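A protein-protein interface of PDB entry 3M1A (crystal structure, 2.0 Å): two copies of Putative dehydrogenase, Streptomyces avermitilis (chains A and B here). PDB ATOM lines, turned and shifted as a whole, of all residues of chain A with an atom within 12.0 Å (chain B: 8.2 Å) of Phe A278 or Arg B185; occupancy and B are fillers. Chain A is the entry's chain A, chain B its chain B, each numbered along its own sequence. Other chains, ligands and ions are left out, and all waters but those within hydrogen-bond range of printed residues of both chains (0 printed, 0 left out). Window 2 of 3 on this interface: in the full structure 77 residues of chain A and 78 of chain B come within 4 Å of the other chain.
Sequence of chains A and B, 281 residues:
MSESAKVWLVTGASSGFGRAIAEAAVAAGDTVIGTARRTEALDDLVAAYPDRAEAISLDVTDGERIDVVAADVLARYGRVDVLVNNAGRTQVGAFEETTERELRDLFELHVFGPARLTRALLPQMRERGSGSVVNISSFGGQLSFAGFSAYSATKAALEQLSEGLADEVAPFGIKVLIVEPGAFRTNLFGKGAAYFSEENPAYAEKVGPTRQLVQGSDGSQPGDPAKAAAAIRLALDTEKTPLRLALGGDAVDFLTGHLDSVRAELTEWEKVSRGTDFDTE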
ATOM      1  N   LYS A 271     -11.749  -2.859   1.529  1.00  0.00           N
ATOM      2  CA  LYS A 271     -12.528  -4.084   1.433  1.00  0.00           C
ATOM      3  C   LYS A 271     -13.493  -4.234   2.604  1.00  0.00           C
ATOM      4  O   LYS A 271     -14.668  -4.554   2.395  1.00  0.00           O
ATOM      5  CB  LYS A 271     -11.625  -5.315   1.259  1.00  0.00           C
ATOM      6  CG  LYS A 271     -11.290  -5.575  -0.199  1.00  0.00           C
ATOM      7  CD  LYS A 271     -10.425  -6.811  -0.404  1.00  0.00           C
ATOM      8  CE  LYS A 271      -9.997  -6.925  -1.874  1.00  0.00           C
ATOM      9  NZ  LYS A 271      -9.094  -5.788  -2.277  1.00  0.00           N
ATOM     10  N   VAL A 272     -13.006  -3.948   3.813  1.00  0.00           N
ATOM     11  CA  VAL A 272     -13.854  -3.897   5.004  1.00  0.00           C
ATOM     12  C   VAL A 272     -14.927  -2.786   4.887  1.00  0.00           C
ATOM     13  O   VAL A 272     -16.108  -3.047   5.102  1.00  0.00           O
ATOM     14  CB  VAL A 272     -13.023  -3.792   6.299  1.00  0.00           C
ATOM     15  CG1 VAL A 272     -13.906  -3.525   7.483  1.00  0.00           C
ATOM     16  CG2 VAL A 272     -12.191  -5.106   6.551  1.00  0.00           C
ATOM     17  N   SER A 273     -14.514  -1.584   4.489  1.00  0.00           N
ATOM     18  CA  SER A 273     -15.429  -0.464   4.279  1.00  0.00           C
ATOM     19  C   SER A 273     -16.592  -0.793   3.334  1.00  0.00           C
ATOM     20  O   SER A 273     -17.757  -0.474   3.622  1.00  0.00           O
ATOM     21  CB  SER A 273     -14.657   0.775   3.790  1.00  0.00           C
ATOM     22  OG  SER A 273     -13.690   1.173   4.772  1.00  0.00           O
ATOM     23  N   ARG A 274     -16.280  -1.457   2.231  1.00  0.00           N
ATOM     24  CA  ARG A 274     -17.280  -1.776   1.215  1.00  0.00           C
ATOM     25  C   ARG A 274     -18.178  -2.973   1.582  1.00  0.00           C
ATOM     26  O   ARG A 274     -19.235  -3.148   0.992  1.00  0.00           O
ATOM     27  CB  ARG A 274     -16.616  -1.939  -0.167  1.00  0.00           C
ATOM     28  CG  ARG A 274     -16.111  -0.605  -0.767  1.00  0.00           C
ATOM     29  CD  ARG A 274     -15.458  -0.753  -2.155  1.00  0.00           C
ATOM     30  NE  ARG A 274     -15.001   0.525  -2.710  1.00  0.00           N
ATOM     31  CZ  ARG A 274     -15.811   1.465  -3.209  1.00  0.00           C
ATOM     32  NH1 ARG A 274     -15.319   2.583  -3.709  1.00  0.00           N
ATOM     33  NH2 ARG A 274     -17.118   1.273  -3.238  1.00  0.00           N
ATOM     34  N   GLY A 275     -17.782  -3.772   2.575  1.00  0.00           N
ATOM     35  CA  GLY A 275     -18.512  -4.994   2.890  1.00  0.00           C
ATOM     36  C   GLY A 275     -19.659  -4.852   3.877  1.00  0.00           C
ATOM     37  O   GLY A 275     -20.216  -5.849   4.314  1.00  0.00           O
ATOM     38  N   THR A 276     -20.032  -3.619   4.215  1.00  0.00           N
ATOM     39  CA  THR A 276     -21.118  -3.369   5.162  1.00  0.00           C
ATOM     40  C   THR A 276     -22.505  -3.212   4.520  1.00  0.00           C
ATOM     41  O   THR A 276     -23.493  -2.995   5.226  1.00  0.00           O
ATOM     42  CB  THR A 276     -20.807  -2.162   6.081  1.00  0.00           C
ATOM     43  OG1 THR A 276     -20.607  -0.988   5.288  1.00  0.00           O
ATOM     44  CG2 THR A 276     -19.559  -2.429   6.921  1.00  0.00           C
ATOM     45  N   ASP A 277     -22.599  -3.344   3.195  1.00  0.00           N
ATOM     46  CA  ASP A 277     -23.908  -3.299   2.515  1.00  0.00           C
ATOM     47  C   ASP A 277     -24.906  -4.380   2.943  1.00  0.00           C
ATOM     48  O   ASP A 277     -24.559  -5.558   3.048  1.00  0.00           O
ATOM     49  CB  ASP A 277     -23.736  -3.336   0.997  1.00  0.00           C
ATOM     50  CG  ASP A 277     -23.192  -2.028   0.440  1.00  0.00           C
ATOM     51  OD1 ASP A 277     -22.970  -1.061   1.210  1.00  0.00           O
ATOM     52  OD2 ASP A 277     -22.986  -1.967  -0.788  1.00  0.00           O
ATOM     53  N   PHE A 278     -26.140  -3.949   3.200  1.00  0.00           N
ATOM     54  CA  PHE A 278     -27.243  -4.829   3.554  1.00  0.00           C
ATOM     55  C   PHE A 278     -27.642  -5.671   2.347  1.00  0.00           C
ATOM     56  O   PHE A 278     -27.619  -6.893   2.423  1.00  0.00           O
ATOM     57  CB  PHE A 278     -28.452  -4.013   4.037  1.00  0.00           C
ATOM     58  CG  PHE A 278     -29.507  -4.837   4.718  1.00  0.00           C
ATOM     59  CD1 PHE A 278     -30.451  -5.558   3.974  1.00  0.00           C
ATOM     60  CD2 PHE A 278     -29.575  -4.887   6.113  1.00  0.00           C
ATOM     61  CE1 PHE A 278     -31.449  -6.326   4.608  1.00  0.00           C
ATOM     62  CE2 PHE A 278     -30.572  -5.651   6.761  1.00  0.00           C
ATOM     63  CZ  PHE A 278     -31.506  -6.371   6.008  1.00  0.00           C
ATOM     64  N   GLY B  16     -29.304   3.732  15.928  1.00  0.00           N
ATOM     65  CA  GLY B  16     -28.204   3.782  14.964  1.00  0.00           C
ATOM     66  C   GLY B  16     -27.029   2.898  15.322  1.00  0.00           C
ATOM     67  O   GLY B  16     -27.210   1.786  15.829  1.00  0.00           O
ATOM     68  N   PHE B  17     -25.826   3.403  15.042  1.00  0.00           N
ATOM     69  CA  PHE B  17     -24.576   2.742  15.402  1.00  0.00           C
ATOM     70  C   PHE B  17     -24.413   2.447  16.877  1.00  0.00           C
ATOM     71  O   PHE B  17     -23.838   1.416  17.235  1.00  0.00           O
ATOM     72  CB  PHE B  17     -23.380   3.561  14.918  1.00  0.00           C
ATOM     73  CG  PHE B  17     -23.047   3.326  13.489  1.00  0.00           C
ATOM     74  CD1 PHE B  17     -21.731   3.209  13.084  1.00  0.00           C
ATOM     75  CD2 PHE B  17     -24.055   3.178  12.546  1.00  0.00           C
ATOM     76  CE1 PHE B  17     -21.445   2.988  11.749  1.00  0.00           C
ATOM     77  CE2 PHE B  17     -23.785   2.952  11.224  1.00  0.00           C
ATOM     78  CZ  PHE B  17     -22.484   2.857  10.816  1.00  0.00           C
ATOM     79  N   GLY B 182     -21.387   6.068   5.777  1.00  0.00           N
ATOM     80  CA  GLY B 182     -22.222   6.636   4.751  1.00  0.00           C
ATOM     81  C   GLY B 182     -23.668   6.344   5.144  1.00  0.00           C
ATOM     82  O   GLY B 182     -24.025   6.470   6.302  1.00  0.00           O
ATOM     83  N   ALA B 183     -24.487   5.932   4.186  1.00  0.00           N
ATOM     84  CA  ALA B 183     -25.926   5.802   4.440  1.00  0.00           C
ATOM     85  C   ALA B 183     -26.297   4.403   4.970  1.00  0.00           C
ATOM     86  O   ALA B 183     -25.974   3.385   4.347  1.00  0.00           O
ATOM     87  CB  ALA B 183     -26.717   6.150   3.153  1.00  0.00           C
ATOM     88  N   PHE B 184     -26.983   4.366   6.105  1.00  0.00           N
ATOM     89  CA  PHE B 184     -27.343   3.105   6.776  1.00  0.00           C
ATOM     90  C   PHE B 184     -28.845   2.938   6.990  1.00  0.00           C
ATOM     91  O   PHE B 184     -29.541   3.932   7.238  1.00  0.00           O
ATOM     92  CB  PHE B 184     -26.560   2.964   8.092  1.00  0.00           C
ATOM     93  CG  PHE B 184     -25.191   2.420   7.867  1.00  0.00           C
ATOM     94  CD1 PHE B 184     -24.204   3.223   7.319  1.00  0.00           C
ATOM     95  CD2 PHE B 184     -24.925   1.081   8.095  1.00  0.00           C
ATOM     96  CE1 PHE B 184     -22.925   2.699   7.024  1.00  0.00           C
ATOM     97  CE2 PHE B 184     -23.673   0.553   7.825  1.00  0.00           C
ATOM     98  CZ  PHE B 184     -22.671   1.361   7.276  1.00  0.00           C
ATOM     99  N   ARG B 185     -29.330   1.696   6.876  1.00  0.00           N
ATOM    100  CA  ARG B 185     -30.746   1.373   7.086  1.00  0.00           C
ATOM    101  C   ARG B 185     -31.109   1.740   8.507  1.00  0.00           C
ATOM    102  O   ARG B 185     -30.288   1.578   9.414  1.00  0.00           O
ATOM    103  CB  ARG B 185     -31.031  -0.123   6.892  1.00  0.00           C
ATOM    104  CG  ARG B 185     -30.755  -0.655   5.495  1.00  0.00           C
ATOM    105  CD  ARG B 185     -31.985  -0.523   4.620  1.00  0.00           C
ATOM    106  NE  ARG B 185     -31.768  -1.137   3.312  1.00  0.00           N
ATOM    107  CZ  ARG B 185     -32.122  -2.379   2.983  1.00  0.00           C
ATOM    108  NH1 ARG B 185     -32.734  -3.167   3.869  1.00  0.00           N
ATOM    109  NH2 ARG B 185     -31.871  -2.829   1.755  1.00  0.00           N
ATOM    110  N   THR B 186     -32.339   2.191   8.706  1.00  0.00           N
ATOM    111  CA  THR B 186     -32.775   2.629  10.024  1.00  0.00           C
ATOM    112  C   THR B 186     -33.980   1.864  10.555  1.00  0.00           C
ATOM    113  O   THR B 186     -34.402   2.096  11.675  1.00  0.00           O
ATOM    114  CB  THR B 186     -33.150   4.136  10.022  1.00  0.00           C
ATOM    115  OG1 THR B 186     -34.359   4.328   9.283  1.00  0.00           O
ATOM    116  CG2 THR B 186     -32.036   4.988   9.420  1.00  0.00           C
ATOM    117  N   ASN B 187     -34.531   0.954   9.758  1.00  0.00           N
ATOM    118  CA  ASN B 187     -35.754   0.254  10.167  1.00  0.00           C
ATOM    119  C   ASN B 187     -35.542  -0.753  11.317  1.00  0.00           C
ATOM    120  O   ASN B 187     -36.470  -1.024  12.079  1.00  0.00           O
ATOM    121  CB  ASN B 187     -36.419  -0.415   8.957  1.00  0.00           C
ATOM    122  CG  ASN B 187     -35.570  -1.520   8.370  1.00  0.00           C
ATOM    123  OD1 ASN B 187     -34.492  -1.278   7.793  1.00  0.00           O
ATOM    124  ND2 ASN B 187     -36.036  -2.754   8.534  1.00  0.00           N
ATOM    125  N   LEU B 188     -34.321  -1.278  11.468  1.00  0.00           N
ATOM    126  CA  LEU B 188     -34.056  -2.220  12.578  1.00  0.00           C
ATOM    127  C   LEU B 188     -33.308  -1.607  13.765  1.00  0.00           C
ATOM    128  O   LEU B 188     -33.460  -2.064  14.891  1.00  0.00           O
ATOM    129  CB  LEU B 188     -33.347  -3.495  12.085  1.00  0.00           C
ATOM    130  CG  LEU B 188     -34.074  -4.298  10.982  1.00  0.00           C
ATOM    131  CD1 LEU B 188     -33.219  -5.456  10.405  1.00  0.00           C
ATOM    132  CD2 LEU B 188     -35.498  -4.800  11.412  1.00  0.00           C
ATOM    133  N   PHE B 189     -32.505  -0.576  13.511  1.00  0.00           N
ATOM    134  CA  PHE B 189     -31.718   0.071  14.567  1.00  0.00           C
ATOM    135  C   PHE B 189     -32.191   1.496  14.876  1.00  0.00           C
ATOM    136  O   PHE B 189     -31.809   2.074  15.911  1.00  0.00           O
ATOM    137  CB  PHE B 189     -30.202   0.012  14.242  1.00  0.00           C
ATOM    138  CG  PHE B 189     -29.630  -1.386  14.341  1.00  0.00           C
ATOM    139  CD1 PHE B 189     -29.236  -1.905  15.571  1.00  0.00           C
ATOM    140  CD2 PHE B 189     -29.557  -2.210  13.217  1.00  0.00           C
ATOM    141  CE1 PHE B 189     -28.737  -3.209  15.679  1.00  0.00           C
ATOM    142  CE2 PHE B 189     -29.055  -3.529  13.312  1.00  0.00           C
ATOM    143  CZ  PHE B 189     -28.644  -4.030  14.546  1.00  0.00           C
ATOM    144  N   GLY B 190     -33.034   2.057  14.003  1.00  0.00           N
ATOM    145  CA  GLY B 190     -33.522   3.436  14.172  1.00  0.00           C
ATOM    146  C   GLY B 190     -32.436   4.452  13.921  1.00  0.00           C
ATOM    147  O   GLY B 190     -31.385   4.132  13.335  1.00  0.00           O
ATOM    148  N   LYS B 191     -32.674   5.682  14.338  1.00  0.00           N
ATOM    149  CA  LYS B 191     -31.668   6.731  14.160  1.00  0.00           C
ATOM    150  C   LYS B 191     -32.001   7.982  14.952  1.00  0.00           C
ATOM    151  O   LYS B 191     -33.080   8.082  15.524  1.00  0.00           O
ATOM    152  CB  LYS B 191     -31.436   7.067  12.676  1.00  0.00           C
ATOM    153  CG  LYS B 191     -32.486   7.951  12.052  1.00  0.00           C
ATOM    154  CD  LYS B 191     -31.921   8.556  10.760  1.00  0.00           C
ATOM    155  CE  LYS B 191     -32.738   9.717  10.294  1.00  0.00           C
ATOM    156  NZ  LYS B 191     -32.011  10.432   9.200  1.00  0.00           N
ATOM    157  N   GLN B 221     -30.019   3.672   3.552  1.00  0.00           N
ATOM    158  CA  GLN B 221     -30.480   2.612   2.649  1.00  0.00           C
ATOM    159  C   GLN B 221     -29.482   1.480   2.334  1.00  0.00           C
ATOM    160  O   GLN B 221     -29.803   0.334   2.575  1.00  0.00           O
ATOM    161  CB  GLN B 221     -31.125   3.200   1.384  1.00  0.00           C
ATOM    162  CG  GLN B 221     -31.626   2.167   0.390  1.00  0.00           C
ATOM    163  CD  GLN B 221     -33.056   2.432  -0.031  1.00  0.00           C
ATOM    164  OE1 GLN B 221     -33.306   3.107  -1.031  1.00  0.00           O
ATOM    165  NE2 GLN B 221     -34.006   1.928   0.751  1.00  0.00           N
ATOM    166  N   PRO B 222     -28.291   1.775   1.770  1.00  0.00           N
ATOM    167  CA  PRO B 222     -27.471   0.578   1.476  1.00  0.00           C
ATOM    168  C   PRO B 222     -26.885  -0.168   2.693  1.00  0.00           C
ATOM    169  O   PRO B 222     -26.735  -1.390   2.636  1.00  0.00           O
ATOM    170  CB  PRO B 222     -26.344   1.114   0.567  1.00  0.00           C
ATOM    171  CG  PRO B 222     -26.358   2.594   0.741  1.00  0.00           C
ATOM    172  CD  PRO B 222     -27.765   2.980   1.100  1.00  0.00           C
ATOM    173  N   GLY B 223     -26.584   0.544   3.781  1.00  0.00           N
ATOM    174  CA  GLY B 223     -25.737  -0.017   4.853  1.00  0.00           C
ATOM    175  C   GLY B 223     -26.423  -0.793   5.955  1.00  0.00           C
ATOM    176  O   GLY B 223     -27.492  -0.410   6.420  1.00  0.00           O
ATOM    177  N   ASP B 224     -25.789  -1.883   6.390  1.00  0.00           N
ATOM    178  CA  ASP B 224     -26.285  -2.704   7.501  1.00  0.00           C
ATOM    179  C   ASP B 224     -25.549  -2.299   8.782  1.00  0.00           C
ATOM    180  O   ASP B 224     -24.340  -2.507   8.886  1.00  0.00           O
ATOM    181  CB  ASP B 224     -26.052  -4.205   7.163  1.00  0.00           C
ATOM    182  CG  ASP B 224     -26.597  -5.180   8.226  1.00  0.00           C
ATOM    183  OD1 ASP B 224     -26.653  -6.404   7.927  1.00  0.00           O
ATOM    184  OD2 ASP B 224     -26.958  -4.759   9.349  1.00  0.00           O
ATOM    185  N   PRO B 225     -26.256  -1.707   9.770  1.00  0.00           N
ATOM    186  CA  PRO B 225     -25.571  -1.286  11.021  1.00  0.00           C
ATOM    187  C   PRO B 225     -24.955  -2.443  11.824  1.00  0.00           C
ATOM    188  O   PRO B 225     -24.003  -2.216  12.562  1.00  0.00           O
ATOM    189  CB  PRO B 225     -26.691  -0.628  11.836  1.00  0.00           C
ATOM    190  CG  PRO B 225     -27.713  -0.195  10.768  1.00  0.00           C
ATOM    191  CD  PRO B 225     -27.669  -1.279   9.746  1.00  0.00           C
ATOM    192  N   ALA B 226     -25.503  -3.658  11.704  1.00  0.00           N
ATOM    193  CA  ALA B 226     -24.931  -4.828  12.397  1.00  0.00           C
ATOM    194  C   ALA B 226     -23.561  -5.144  11.811  1.00  0.00           C
ATOM    195  O   ALA B 226     -22.625  -5.423  12.543  1.00  0.00           O
ATOM    196  CB  ALA B 226     -25.862  -6.063  12.337  1.00  0.00           C
ATOM    197  N   LYS B 227     -23.442  -5.060  10.489  1.00  0.00           N
ATOM    198  CA  LYS B 227     -22.150  -5.234   9.826  1.00  0.00           C
ATOM    199  C   LYS B 227     -21.161  -4.102  10.122  1.00  0.00           C
ATOM    200  O   LYS B 227     -19.936  -4.326  10.149  1.00  0.00           O
ATOM    201  CB  LYS B 227     -22.330  -5.394   8.317  1.00  0.00           C
ATOM    202  CG  LYS B 227     -22.939  -6.712   7.920  1.00  0.00           C
ATOM    203  CD  LYS B 227     -23.055  -6.798   6.413  1.00  0.00           C
ATOM    204  CE  LYS B 227     -23.660  -8.130   5.963  1.00  0.00           C
ATOM    205  NZ  LYS B 227     -23.888  -8.115   4.491  1.00  0.00           N
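The backbone carbonyl oxygen (O) of Thr A276 sits at hydrogen-bond distance from the backbone NH (N) of Asp B224 (2.8 Å). The backbone carbonyl oxygen of Asp A277 sits at hydrogen-bond distance from the side-chain amino group of Lys B227, at 3.0 Å. The backbone NH (N) of Phe A278 lies within hydrogen-bond range of the backbone carbonyl oxygen (O) of Pro B222 (2.7 Å).
OG1 of Thr A276 lies within hydrogen-bond range of O of Ser A273. The backbone NH (N) of Gly B223 sits at hydrogen-bond distance from the backbone carbonyl oxygen (O) of Ala B183. The guanidinium group of Arg B185 is in hydrogen-bond range of the backbone carbonyl oxygen of Gln B221. O of Gly B223 sits at hydrogen-bond distance from N of Arg B185, at 2.8 Å. The side-chain carboxylate (OD2) of Asp B224 lies within hydrogen-bond range of the backbone NH (N) of Ala B226, 3.0 Å away.
CD of Lys B227 touches O of Gly A275, 3.7 Å away. Phe B184 touches Thr A276. Thr A276 touches Gly B223. CG2 of Thr A276 touches O of Lys B227, at 3.8 Å. Asp A277 touches Pro B222. Phe A278 touches Arg B185. CD2 of Phe A278 touches CG of Asp B224 (3.7 Å).
Printed residues of chain B within 4 Å of Gly A275: Lys B227 (3.7 Å). Of the printed residues of chain B, Thr A276 touches Phe B184, Gly B223, Asp B224 and Lys B227. Of the printed residues of chain B, Asp A277 touches Pro B222 (3.4 Å) and Lys B227 (3.0 Å). Gly B16 touches none of the printed residues of chain A. No residue of chain A comes within 4 Å of Ala B183. Phe B184 touches just one residue of chain A: Thr A276. Arg B185 touches just one residue of chain A: Phe A278 (3.3 Å). No residue of chain A comes within 4 Å of Thr B186. Asn B187 touches none of the printed residues of chain A. No residue of chain A comes within 4 Å of Leu B188. No residue of chain A comes within 4 Å of Gly B190. Pro B222 touches two residues of chain A. Of chain A, only Thr A276 comes within 4 Å of Gly B223. Of the printed residues of chain A, Lys B227 touches Gly A275, Thr A276 and Asp A277. The nearest residue of chain B that does not touch Phe A278 is Gly B223 (4.2 Å). The nearest printed residue of chain B that does not touch Thr A276 is Pro B222 (4.4 Å).
Printed residues of chain A that touch a printed residue of chain B: Gly A275, Thr A276, Asp A277 and Phe A278. Hydrophobic or aromatic side chains of chain A that line the printed part of chain B: Phe A278. Of the 19 printed residues of chain B, 6 touch a printed residue of chain A. Printed residues of chain B that touch a printed residue of chain A: Phe B184, Arg B185, Pro B222, Gly B223, Asp B224 and Lys B227. Hydrophobic or aromatic side chains of chain B within 4 Å of the printed part of chain A: Phe B184. Among the printed residues, 10 pairs touch across the chains.
No position is printed for both chains. Of the 10 pairs that touch across the chains among the printed residues, none has its exchanged pair printed and touching as well.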
